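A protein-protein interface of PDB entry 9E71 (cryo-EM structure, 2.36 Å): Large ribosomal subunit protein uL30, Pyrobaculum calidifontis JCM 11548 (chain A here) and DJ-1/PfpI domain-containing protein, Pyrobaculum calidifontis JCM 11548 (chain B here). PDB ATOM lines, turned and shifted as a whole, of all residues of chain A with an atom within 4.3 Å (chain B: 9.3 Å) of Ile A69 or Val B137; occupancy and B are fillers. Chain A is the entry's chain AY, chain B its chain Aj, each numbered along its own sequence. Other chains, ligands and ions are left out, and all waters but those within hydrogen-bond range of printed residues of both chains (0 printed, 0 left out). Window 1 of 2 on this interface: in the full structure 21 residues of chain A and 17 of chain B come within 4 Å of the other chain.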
ATOM      1  N   ARG A  13       2.626 -28.203 -33.248  1.00  0.00           N
ATOM      2  CA  ARG A  13       3.562 -29.060 -32.533  1.00  0.00           C
ATOM      3  C   ARG A  13       3.004 -30.473 -32.484  1.00  0.00           C
ATOM      4  O   ARG A  13       1.912 -30.696 -31.956  1.00  0.00           O
ATOM      5  CB  ARG A  13       3.819 -28.534 -31.125  1.00  0.00           C
ATOM      6  CG  ARG A  13       4.968 -27.567 -31.052  1.00  0.00           C
ATOM      7  CD  ARG A  13       4.534 -26.166 -31.405  1.00  0.00           C
ATOM      8  NE  ARG A  13       5.555 -25.193 -31.046  1.00  0.00           N
ATOM      9  CZ  ARG A  13       6.068 -24.303 -31.882  1.00  0.00           C
ATOM     10  NH1 ARG A  13       5.657 -24.216 -33.135  1.00  0.00           N
ATOM     11  NH2 ARG A  13       7.016 -23.480 -31.449  1.00  0.00           N
ATOM     12  N   TYR A  14       3.761 -31.422 -33.014  1.00  0.00           N
ATOM     13  CA  TYR A  14       3.299 -32.785 -33.197  1.00  0.00           C
ATOM     14  C   TYR A  14       4.056 -33.748 -32.297  1.00  0.00           C
ATOM     15  O   TYR A  14       5.246 -33.577 -32.024  1.00  0.00           O
ATOM     16  CB  TYR A  14       3.458 -33.224 -34.650  1.00  0.00           C
ATOM     17  CG  TYR A  14       2.563 -32.494 -35.613  1.00  0.00           C
ATOM     18  CD1 TYR A  14       1.203 -32.742 -35.648  1.00  0.00           C
ATOM     19  CD2 TYR A  14       3.080 -31.559 -36.491  1.00  0.00           C
ATOM     20  CE1 TYR A  14       0.384 -32.079 -36.529  1.00  0.00           C
ATOM     21  CE2 TYR A  14       2.268 -30.894 -37.375  1.00  0.00           C
ATOM     22  CZ  TYR A  14       0.924 -31.156 -37.390  1.00  0.00           C
ATOM     23  OH  TYR A  14       0.113 -30.489 -38.272  1.00  0.00           O
ATOM     24  N   ALA A  15       3.341 -34.762 -31.839  1.00  0.00           N
ATOM     25  CA  ALA A  15       3.931 -35.916 -31.184  1.00  0.00           C
ATOM     26  C   ALA A  15       4.028 -37.043 -32.199  1.00  0.00           C
ATOM     27  O   ALA A  15       3.061 -37.317 -32.917  1.00  0.00           O
ATOM     28  CB  ALA A  15       3.100 -36.353 -29.979  1.00  0.00           C
ATOM     29  N   VAL A  46       8.704 -34.844 -29.881  1.00  0.00           N
ATOM     30  CA  VAL A  46       7.841 -33.695 -30.116  1.00  0.00           C
ATOM     31  C   VAL A  46       8.567 -32.774 -31.082  1.00  0.00           C
ATOM     32  O   VAL A  46       9.708 -32.373 -30.830  1.00  0.00           O
ATOM     33  CB  VAL A  46       7.494 -32.970 -28.810  1.00  0.00           C
ATOM     34  CG1 VAL A  46       6.279 -32.099 -29.008  1.00  0.00           C
ATOM     35  CG2 VAL A  46       7.247 -33.972 -27.712  1.00  0.00           C
ATOM     36  N   GLY A  67       0.428 -37.010 -34.196  1.00  0.00           N
ATOM     37  CA  GLY A  67      -0.747 -36.190 -33.973  1.00  0.00           C
ATOM     38  C   GLY A  67      -0.363 -34.865 -33.367  1.00  0.00           C
ATOM     39  O   GLY A  67       0.813 -34.568 -33.165  1.00  0.00           O
ATOM     40  N   GLU A  68      -1.380 -34.057 -33.085  1.00  0.00           N
ATOM     41  CA  GLU A  68      -1.174 -32.767 -32.439  1.00  0.00           C
ATOM     42  C   GLU A  68      -1.244 -32.965 -30.933  1.00  0.00           C
ATOM     43  O   GLU A  68      -2.294 -33.330 -30.397  1.00  0.00           O
ATOM     44  CB  GLU A  68      -2.215 -31.758 -32.910  1.00  0.00           C
ATOM     45  CG  GLU A  68      -2.344 -31.673 -34.413  1.00  0.00           C
ATOM     46  CD  GLU A  68      -3.485 -32.509 -34.938  1.00  0.00           C
ATOM     47  OE1 GLU A  68      -4.004 -33.344 -34.174  1.00  0.00           O
ATOM     48  OE2 GLU A  68      -3.860 -32.340 -36.116  1.00  0.00           O
ATOM     49  N   ILE A  69      -0.132 -32.733 -30.255  1.00  0.00           N
ATOM     50  CA  ILE A  69      -0.042 -32.939 -28.815  1.00  0.00           C
ATOM     51  C   ILE A  69      -0.545 -31.700 -28.088  1.00  0.00           C
ATOM     52  O   ILE A  69      -0.323 -30.567 -28.521  1.00  0.00           O
ATOM     53  CB  ILE A  69       1.407 -33.280 -28.420  1.00  0.00           C
ATOM     54  CG1 ILE A  69       1.524 -33.481 -26.912  1.00  0.00           C
ATOM     55  CG2 ILE A  69       2.344 -32.191 -28.885  1.00  0.00           C
ATOM     56  CD1 ILE A  69       2.603 -34.438 -26.512  1.00  0.00           C
ATOM     57  N   ASP A  70      -1.235 -31.914 -26.971  1.00  0.00           N
ATOM     58  CA  ASP A  70      -1.766 -30.831 -26.162  1.00  0.00           C
ATOM     59  C   ASP A  70      -0.849 -30.554 -24.978  1.00  0.00           C
ATOM     60  O   ASP A  70      -0.024 -31.386 -24.592  1.00  0.00           O
ATOM     61  CB  ASP A  70      -3.182 -31.151 -25.674  1.00  0.00           C
ATOM     62  CG  ASP A  70      -3.195 -31.946 -24.389  1.00  0.00           C
ATOM     63  OD1 ASP A  70      -3.185 -33.189 -24.465  1.00  0.00           O
ATOM     64  OD2 ASP A  70      -3.231 -31.332 -23.304  1.00  0.00           O
ATOM     65  N   LEU A  74       1.610 -32.952 -22.744  1.00  0.00           N
ATOM     66  CA  LEU A  74       3.044 -32.690 -22.758  1.00  0.00           C
ATOM     67  C   LEU A  74       3.589 -32.490 -21.350  1.00  0.00           C
ATOM     68  O   LEU A  74       4.679 -32.973 -21.029  1.00  0.00           O
ATOM     69  CB  LEU A  74       3.350 -31.474 -23.628  1.00  0.00           C
ATOM     70  CG  LEU A  74       4.836 -31.138 -23.761  1.00  0.00           C
ATOM     71  CD1 LEU A  74       5.633 -32.389 -24.062  1.00  0.00           C
ATOM     72  CD2 LEU A  74       5.061 -30.095 -24.835  1.00  0.00           C
ATOM     73  N   ILE A 111       3.894 -25.427 -26.594  1.00  0.00           N
ATOM     74  CA  ILE A 111       2.765 -25.722 -27.470  1.00  0.00           C
ATOM     75  C   ILE A 111       2.224 -24.445 -28.102  1.00  0.00           C
ATOM     76  O   ILE A 111       1.905 -24.413 -29.295  1.00  0.00           O
ATOM     77  CB  ILE A 111       1.667 -26.479 -26.709  1.00  0.00           C
ATOM     78  CG1 ILE A 111       2.200 -27.812 -26.200  1.00  0.00           C
ATOM     79  CG2 ILE A 111       0.488 -26.724 -27.617  1.00  0.00           C
ATOM     80  CD1 ILE A 111       2.615 -28.748 -27.292  1.00  0.00           C
ATOM     81  N   ASN A 172      -3.047 -37.948 -28.047  1.00  0.00           N
ATOM     82  CA  ASN A 172      -3.013 -37.669 -26.616  1.00  0.00           C
ATOM     83  C   ASN A 172      -3.595 -38.823 -25.809  1.00  0.00           C
ATOM     84  O   ASN A 172      -3.051 -39.186 -24.758  1.00  0.00           O
ATOM     85  CB  ASN A 172      -3.758 -36.372 -26.332  1.00  0.00           C
ATOM     86  CG  ASN A 172      -3.132 -35.191 -27.027  1.00  0.00           C
ATOM     87  OD1 ASN A 172      -2.009 -34.803 -26.721  1.00  0.00           O
ATOM     88  ND2 ASN A 172      -3.847 -34.624 -27.985  1.00  0.00           N
ATOM     89  N   ILE A 175      -1.018 -41.466 -25.856  1.00  0.00           N
ATOM     90  CA  ILE A 175       0.107 -41.144 -24.989  1.00  0.00           C
ATOM     91  C   ILE A 175      -0.250 -41.389 -23.531  1.00  0.00           C
ATOM     92  O   ILE A 175       0.584 -41.850 -22.743  1.00  0.00           O
ATOM     93  CB  ILE A 175       0.562 -39.694 -25.224  1.00  0.00           C
ATOM     94  CG1 ILE A 175       1.234 -39.568 -26.589  1.00  0.00           C
ATOM     95  CG2 ILE A 175       1.513 -39.259 -24.130  1.00  0.00           C
ATOM     96  CD1 ILE A 175       1.258 -38.162 -27.126  1.00  0.00           C
ATOM     97  N   TYR B  75     -13.725 -30.050 -34.143  1.00  0.00           N
ATOM     98  CA  TYR B  75     -12.304 -29.717 -34.164  1.00  0.00           C
ATOM     99  C   TYR B  75     -11.818 -29.523 -35.594  1.00  0.00           C
ATOM    100  O   TYR B  75     -11.186 -28.511 -35.918  1.00  0.00           O
ATOM    101  CB  TYR B  75     -11.517 -30.805 -33.404  1.00  0.00           C
ATOM    102  CG  TYR B  75      -9.994 -30.865 -33.560  1.00  0.00           C
ATOM    103  CD1 TYR B  75      -9.378 -31.447 -34.669  1.00  0.00           C
ATOM    104  CD2 TYR B  75      -9.174 -30.312 -32.588  1.00  0.00           C
ATOM    105  CE1 TYR B  75      -8.023 -31.472 -34.795  1.00  0.00           C
ATOM    106  CE2 TYR B  75      -7.810 -30.341 -32.710  1.00  0.00           C
ATOM    107  CZ  TYR B  75      -7.243 -30.923 -33.817  1.00  0.00           C
ATOM    108  OH  TYR B  75      -5.880 -30.959 -33.955  1.00  0.00           O
ATOM    109  N   VAL B  78     -13.401 -26.450 -37.243  1.00  0.00           N
ATOM    110  CA  VAL B  78     -12.791 -25.207 -36.786  1.00  0.00           C
ATOM    111  C   VAL B  78     -11.413 -25.026 -37.407  1.00  0.00           C
ATOM    112  O   VAL B  78     -11.041 -23.920 -37.818  1.00  0.00           O
ATOM    113  CB  VAL B  78     -12.722 -25.188 -35.249  1.00  0.00           C
ATOM    114  CG1 VAL B  78     -11.701 -24.173 -34.776  1.00  0.00           C
ATOM    115  CG2 VAL B  78     -14.088 -24.895 -34.663  1.00  0.00           C
ATOM    116  N   LEU B  79     -10.634 -26.105 -37.485  1.00  0.00           N
ATOM    117  CA  LEU B  79      -9.318 -26.019 -38.102  1.00  0.00           C
ATOM    118  C   LEU B  79      -9.391 -25.895 -39.618  1.00  0.00           C
ATOM    119  O   LEU B  79      -8.406 -25.478 -40.234  1.00  0.00           O
ATOM    120  CB  LEU B  79      -8.483 -27.239 -37.721  1.00  0.00           C
ATOM    121  CG  LEU B  79      -7.844 -27.194 -36.334  1.00  0.00           C
ATOM    122  CD1 LEU B  79      -6.937 -28.390 -36.122  1.00  0.00           C
ATOM    123  CD2 LEU B  79      -7.079 -25.904 -36.165  1.00  0.00           C
ATOM    124  N   MET B 115     -13.554 -28.919 -25.347  1.00  0.00           N
ATOM    125  CA  MET B 115     -12.673 -29.223 -26.473  1.00  0.00           C
ATOM    126  C   MET B 115     -12.617 -28.108 -27.510  1.00  0.00           C
ATOM    127  O   MET B 115     -12.254 -26.975 -27.189  1.00  0.00           O
ATOM    128  CB  MET B 115     -13.095 -30.531 -27.142  1.00  0.00           C
ATOM    129  CG  MET B 115     -12.260 -31.726 -26.718  1.00  0.00           C
ATOM    130  SD  MET B 115     -12.098 -32.973 -28.009  1.00  0.00           S
ATOM    131  CE  MET B 115     -11.248 -32.040 -29.280  1.00  0.00           C
ATOM    132  N   ALA B 116     -12.952 -28.420 -28.759  1.00  0.00           N
ATOM    133  CA  ALA B 116     -12.889 -27.445 -29.839  1.00  0.00           C
ATOM    134  C   ALA B 116     -14.110 -26.538 -29.892  1.00  0.00           C
ATOM    135  O   ALA B 116     -14.116 -25.577 -30.672  1.00  0.00           O
ATOM    136  CB  ALA B 116     -12.730 -28.159 -31.182  1.00  0.00           C
ATOM    137  N   ALA B 119     -13.244 -22.956 -29.363  1.00  0.00           N
ATOM    138  CA  ALA B 119     -12.716 -22.368 -30.588  1.00  0.00           C
ATOM    139  C   ALA B 119     -13.838 -22.035 -31.560  1.00  0.00           C
ATOM    140  O   ALA B 119     -13.796 -21.003 -32.238  1.00  0.00           O
ATOM    141  CB  ALA B 119     -11.707 -23.314 -31.232  1.00  0.00           C
ATOM    142  N   THR B 133     -10.992 -21.011 -22.058  1.00  0.00           N
ATOM    143  CA  THR B 133     -10.040 -22.095 -22.223  1.00  0.00           C
ATOM    144  C   THR B 133     -10.513 -23.016 -23.340  1.00  0.00           C
ATOM    145  O   THR B 133     -11.707 -23.135 -23.616  1.00  0.00           O
ATOM    146  CB  THR B 133      -9.860 -22.886 -20.921  1.00  0.00           C
ATOM    147  OG1 THR B 133      -8.556 -23.478 -20.896  1.00  0.00           O
ATOM    148  CG2 THR B 133     -10.901 -23.979 -20.806  1.00  0.00           C
ATOM    149  N   VAL B 134      -9.548 -23.654 -23.999  1.00  0.00           N
ATOM    150  CA  VAL B 134      -9.820 -24.568 -25.101  1.00  0.00           C
ATOM    151  C   VAL B 134      -8.853 -25.734 -24.965  1.00  0.00           C
ATOM    152  O   VAL B 134      -7.975 -25.736 -24.102  1.00  0.00           O
ATOM    153  CB  VAL B 134      -9.677 -23.862 -26.471  1.00  0.00           C
ATOM    154  CG1 VAL B 134      -8.222 -23.773 -26.875  1.00  0.00           C
ATOM    155  CG2 VAL B 134     -10.488 -24.562 -27.537  1.00  0.00           C
ATOM    156  N   TYR B 135      -9.036 -26.749 -25.810  1.00  0.00           N
ATOM    157  CA  TYR B 135      -8.112 -27.872 -25.878  1.00  0.00           C
ATOM    158  C   TYR B 135      -6.740 -27.348 -26.273  1.00  0.00           C
ATOM    159  O   TYR B 135      -6.577 -26.787 -27.362  1.00  0.00           O
ATOM    160  CB  TYR B 135      -8.610 -28.911 -26.881  1.00  0.00           C
ATOM    161  CG  TYR B 135      -7.997 -30.277 -26.716  1.00  0.00           C
ATOM    162  CD1 TYR B 135      -8.018 -30.922 -25.494  1.00  0.00           C
ATOM    163  CD2 TYR B 135      -7.407 -30.924 -27.787  1.00  0.00           C
ATOM    164  CE1 TYR B 135      -7.461 -32.173 -25.341  1.00  0.00           C
ATOM    165  CE2 TYR B 135      -6.850 -32.173 -27.647  1.00  0.00           C
ATOM    166  CZ  TYR B 135      -6.878 -32.794 -26.421  1.00  0.00           C
ATOM    167  OH  TYR B 135      -6.323 -34.042 -26.272  1.00  0.00           O
ATOM    168  N   PRO B 136      -5.735 -27.519 -25.431  1.00  0.00           N
ATOM    169  CA  PRO B 136      -4.482 -26.752 -25.581  1.00  0.00           C
ATOM    170  C   PRO B 136      -3.572 -27.295 -26.674  1.00  0.00           C
ATOM    171  O   PRO B 136      -2.505 -27.865 -26.435  1.00  0.00           O
ATOM    172  CB  PRO B 136      -3.863 -26.859 -24.183  1.00  0.00           C
ATOM    173  CG  PRO B 136      -4.540 -28.007 -23.517  1.00  0.00           C
ATOM    174  CD  PRO B 136      -5.644 -28.523 -24.366  1.00  0.00           C
ATOM    175  N   VAL B 137      -4.002 -27.111 -27.914  1.00  0.00           N
ATOM    176  CA  VAL B 137      -3.164 -27.355 -29.074  1.00  0.00           C
ATOM    177  C   VAL B 137      -2.802 -26.006 -29.678  1.00  0.00           C
ATOM    178  O   VAL B 137      -3.457 -24.987 -29.429  1.00  0.00           O
ATOM    179  CB  VAL B 137      -3.843 -28.265 -30.116  1.00  0.00           C
ATOM    180  CG1 VAL B 137      -3.925 -29.686 -29.595  1.00  0.00           C
ATOM    181  CG2 VAL B 137      -5.225 -27.743 -30.463  1.00  0.00           C
ATOM    182  N   THR B 138      -1.732 -26.012 -30.478  1.00  0.00           N
ATOM    183  CA  THR B 138      -1.195 -24.780 -31.046  1.00  0.00           C
ATOM    184  C   THR B 138      -2.208 -24.094 -31.949  1.00  0.00           C
ATOM    185  O   THR B 138      -2.426 -22.882 -31.856  1.00  0.00           O
ATOM    186  CB  THR B 138       0.078 -25.085 -31.835  1.00  0.00           C
ATOM    187  OG1 THR B 138       1.013 -25.774 -31.000  1.00  0.00           O
ATOM    188  CG2 THR B 138       0.703 -23.807 -32.345  1.00  0.00           C
ATOM    189  N   GLU B 139      -2.860 -24.868 -32.808  1.00  0.00           N
ATOM    190  CA  GLU B 139      -3.765 -24.286 -33.787  1.00  0.00           C
ATOM    191  C   GLU B 139      -5.024 -23.732 -33.127  1.00  0.00           C
ATOM    192  O   GLU B 139      -5.490 -22.643 -33.484  1.00  0.00           O
ATOM    193  CB  GLU B 139      -4.109 -25.333 -34.840  1.00  0.00           C
ATOM    194  CG  GLU B 139      -2.891 -25.994 -35.468  1.00  0.00           C
ATOM    195  CD  GLU B 139      -2.993 -27.507 -35.482  1.00  0.00           C
ATOM    196  OE1 GLU B 139      -2.708 -28.117 -36.533  1.00  0.00           O
ATOM    197  OE2 GLU B 139      -3.354 -28.088 -34.436  1.00  0.00           O
ATOM    198  N   LEU B 140      -5.588 -24.458 -32.162  1.00  0.00           N
ATOM    199  CA  LEU B 140      -6.782 -23.967 -31.481  1.00  0.00           C
ATOM    200  C   LEU B 140      -6.470 -22.751 -30.616  1.00  0.00           C
ATOM    201  O   LEU B 140      -7.274 -21.811 -30.541  1.00  0.00           O
ATOM    202  CB  LEU B 140      -7.405 -25.083 -30.646  1.00  0.00           C
ATOM    203  CG  LEU B 140      -8.063 -26.193 -31.468  1.00  0.00           C
ATOM    204  CD1 LEU B 140      -8.734 -27.221 -30.574  1.00  0.00           C
ATOM    205  CD2 LEU B 140      -9.050 -25.611 -32.454  1.00  0.00           C
ATOM    206  N   ILE B 141      -5.308 -22.751 -29.955  1.00  0.00           N
ATOM    207  CA  ILE B 141      -4.894 -21.581 -29.187  1.00  0.00           C
ATOM    208  C   ILE B 141      -4.710 -20.380 -30.102  1.00  0.00           C
ATOM    209  O   ILE B 141      -5.070 -19.250 -29.751  1.00  0.00           O
ATOM    210  CB  ILE B 141      -3.608 -21.882 -28.397  1.00  0.00           C
ATOM    211  CG1 ILE B 141      -3.893 -22.866 -27.262  1.00  0.00           C
ATOM    212  CG2 ILE B 141      -3.015 -20.601 -27.858  1.00  0.00           C
ATOM    213  CD1 ILE B 141      -2.645 -23.423 -26.612  1.00  0.00           C
ATOM    214  N   LYS B 142      -4.155 -20.608 -31.293  1.00  0.00           N
ATOM    215  CA  LYS B 142      -4.010 -19.529 -32.261  1.00  0.00           C
ATOM    216  C   LYS B 142      -5.366 -19.020 -32.732  1.00  0.00           C
ATOM    217  O   LYS B 142      -5.536 -17.818 -32.947  1.00  0.00           O
ATOM    218  CB  LYS B 142      -3.161 -19.999 -33.440  1.00  0.00           C
ATOM    219  CG  LYS B 142      -2.831 -18.920 -34.461  1.00  0.00           C
ATOM    220  CD  LYS B 142      -2.624 -17.553 -33.831  1.00  0.00           C
ATOM    221  CE  LYS B 142      -1.431 -17.527 -32.899  1.00  0.00           C
ATOM    222  NZ  LYS B 142      -0.760 -16.198 -32.913  1.00  0.00           N
ATOM    223  N   ILE B 143      -6.341 -19.915 -32.904  1.00  0.00           N
ATOM    224  CA  ILE B 143      -7.674 -19.482 -33.321  1.00  0.00           C
ATOM    225  C   ILE B 143      -8.315 -18.607 -32.249  1.00  0.00           C
ATOM    226  O   ILE B 143      -8.931 -17.576 -32.550  1.00  0.00           O
ATOM    227  CB  ILE B 143      -8.560 -20.694 -33.659  1.00  0.00           C
ATOM    228  CG1 ILE B 143      -8.385 -21.080 -35.126  1.00  0.00           C
ATOM    229  CG2 ILE B 143     -10.015 -20.380 -33.376  1.00  0.00           C
ATOM    230  CD1 ILE B 143      -8.845 -20.006 -36.096  1.00  0.00           C
ATOM    231  N   LEU B 144      -8.170 -19.001 -30.982  1.00  0.00           N
ATOM    232  CA  LEU B 144      -8.698 -18.185 -29.890  1.00  0.00           C
ATOM    233  C   LEU B 144      -8.011 -16.823 -29.829  1.00  0.00           C
ATOM    234  O   LEU B 144      -8.669 -15.784 -29.691  1.00  0.00           O
ATOM    235  CB  LEU B 144      -8.546 -18.920 -28.561  1.00  0.00           C
ATOM    236  CG  LEU B 144      -9.821 -19.432 -27.896  1.00  0.00           C
ATOM    237  CD1 LEU B 144     -10.642 -20.258 -28.863  1.00  0.00           C
ATOM    238  CD2 LEU B 144      -9.465 -20.236 -26.662  1.00  0.00           C
ATOM    239  N   ARG B 145      -6.682 -16.807 -29.949  1.00  0.00           N
ATOM    240  CA  ARG B 145      -5.960 -15.543 -29.877  1.00  0.00           C
ATOM    241  C   ARG B 145      -6.263 -14.653 -31.076  1.00  0.00           C
ATOM    242  O   ARG B 145      -6.236 -13.425 -30.955  1.00  0.00           O
ATOM    243  CB  ARG B 145      -4.461 -15.805 -29.768  1.00  0.00           C
ATOM    244  CG  ARG B 145      -4.048 -16.418 -28.446  1.00  0.00           C
ATOM    245  CD  ARG B 145      -2.739 -15.832 -27.963  1.00  0.00           C
ATOM    246  NE  ARG B 145      -1.831 -16.855 -27.458  1.00  0.00           N
ATOM    247  CZ  ARG B 145      -1.788 -17.261 -26.198  1.00  0.00           C
ATOM    248  NH1 ARG B 145      -2.603 -16.764 -25.283  1.00  0.00           N
ATOM    249  NH2 ARG B 145      -0.899 -18.185 -25.844  1.00  0.00           N
ATOM    250  N   PHE B 151      -6.828 -16.504 -23.560  1.00  0.00           N
ATOM    251  CA  PHE B 151      -6.662 -17.905 -23.212  1.00  0.00           C
ATOM    252  C   PHE B 151      -6.222 -18.043 -21.761  1.00  0.00           C
ATOM    253  O   PHE B 151      -5.322 -17.336 -21.302  1.00  0.00           O
ATOM    254  CB  PHE B 151      -5.650 -18.572 -24.138  1.00  0.00           C
ATOM    255  CG  PHE B 151      -5.318 -19.978 -23.749  1.00  0.00           C
ATOM    256  CD1 PHE B 151      -6.276 -20.971 -23.810  1.00  0.00           C
ATOM    257  CD2 PHE B 151      -4.049 -20.308 -23.315  1.00  0.00           C
ATOM    258  CE1 PHE B 151      -5.970 -22.265 -23.447  1.00  0.00           C
ATOM    259  CE2 PHE B 151      -3.743 -21.598 -22.956  1.00  0.00           C
ATOM    260  CZ  PHE B 151      -4.703 -22.576 -23.023  1.00  0.00           C
ATOM    261  N   ASN B 153      -5.175 -21.068 -18.848  1.00  0.00           N
ATOM    262  CA  ASN B 153      -4.691 -22.440 -18.781  1.00  0.00           C
ATOM    263  C   ASN B 153      -5.298 -23.227 -17.624  1.00  0.00           C
ATOM    264  O   ASN B 153      -4.685 -24.181 -17.138  1.00  0.00           O
ATOM    265  CB  ASN B 153      -3.169 -22.460 -18.694  1.00  0.00           C
ATOM    266  CG  ASN B 153      -2.575 -23.725 -19.265  1.00  0.00           C
ATOM    267  OD1 ASN B 153      -3.236 -24.452 -20.008  1.00  0.00           O
ATOM    268  ND2 ASN B 153      -1.323 -24.002 -18.919  1.00  0.00           N
ATOM    269  N   LYS B 166     -11.376 -27.563 -21.044  1.00  0.00           N
ATOM    270  CA  LYS B 166     -10.323 -28.064 -21.919  1.00  0.00           C
ATOM    271  C   LYS B 166     -10.702 -29.415 -22.508  1.00  0.00           C
ATOM    272  O   LYS B 166     -10.611 -29.626 -23.722  1.00  0.00           O
ATOM    273  CB  LYS B 166      -9.006 -28.163 -21.149  1.00  0.00           C
ATOM    274  CG  LYS B 166      -8.275 -26.847 -21.007  1.00  0.00           C
ATOM    275  CD  LYS B 166      -6.778 -27.046 -21.035  1.00  0.00           C
ATOM    276  CE  LYS B 166      -6.202 -27.115 -19.635  1.00  0.00           C
ATOM    277  NZ  LYS B 166      -4.996 -26.259 -19.493  1.00  0.00           N
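Printed residues of chain B that touch a printed residue of chain A: Tyr B75, Tyr B135, Pro B136, Val B137, Thr B138 and Glu B139.
Hydrophobic or aromatic side chains of chain B that line the printed part of chain A: Tyr B75, Tyr B135, Pro B136 and Val B137.
Printed residues of chain A that touch a printed residue of chain B: Arg A13, Glu A68, Ile A69, Asp A70, Ile A111 and Asn A172.
Hydrophobic or aromatic side chains of chain A that line the printed part of chain B: Ile A111.
Among the printed residues, 10 pairs touch across the chains.
Among the printed residues, no Asp or Glu carboxylate lies within 4 Å of a Lys or Arg side-chain nitrogen of the other chain.
The side-chain hydroxyl of Tyr B75 lies close to the side-chain carboxylate of Glu A68, at 3.0 Å.
ND2 of Asn A172 is in hydrogen-bond range of OH of Tyr B135.
The backbone carbonyl oxygen (O) of Ile A111 lies close to the side-chain hydroxyl (OG1) of Thr B138 (2.4 Å).
Among the printed residues, pairs that only touch across the chains: Asp A70 with Pro B136 (3.1 Å), Ile A111 with Pro B136 (3.4 Å), Arg A13 with Thr B138 (3.6 Å), Asp A70 with Tyr B135 (3.7 Å), Glu A68 with Glu B139 (3.7 Å), Ile A69 with Val B137 (3.9 Å) and Ile A111 with Val B137 (3.9 Å).
Of the printed residues of chain B, Ile A69 touches Val B137.
Of the printed residues of chain B, Asp A70 touches Tyr B135 and Pro B136.
Ala B119 touches none of the printed residues of chain A.
Val B137 touches two residues of chain A.
Of the printed residues of chain A, Thr B138 touches Arg A13 (3.6 Å) and Ile A111 (2.4 Å).
Ile B143 touches none of the printed residues of chain A.
The nearest residue of chain B that does not touch Ile A69 is Pro B136 (4.1 Å).
The nearest residue of chain A that does not touch Val B137 is Glu A68 (4.1 Å).
The nearest printed residue of chain B that does not touch Ile A111 is Ile B141 (4.7 Å).
OD1 of Asn A172 lies within hydrogen-bond range of N of Asp A70 (3.0 Å).
N of Ile A69 is in hydrogen-bond range of O of Arg A13, 3.3 Å away.
The side-chain amide nitrogen of Asn A172 sits at hydrogen-bond distance from the backbone carbonyl oxygen of Glu A68 (3.1 Å).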
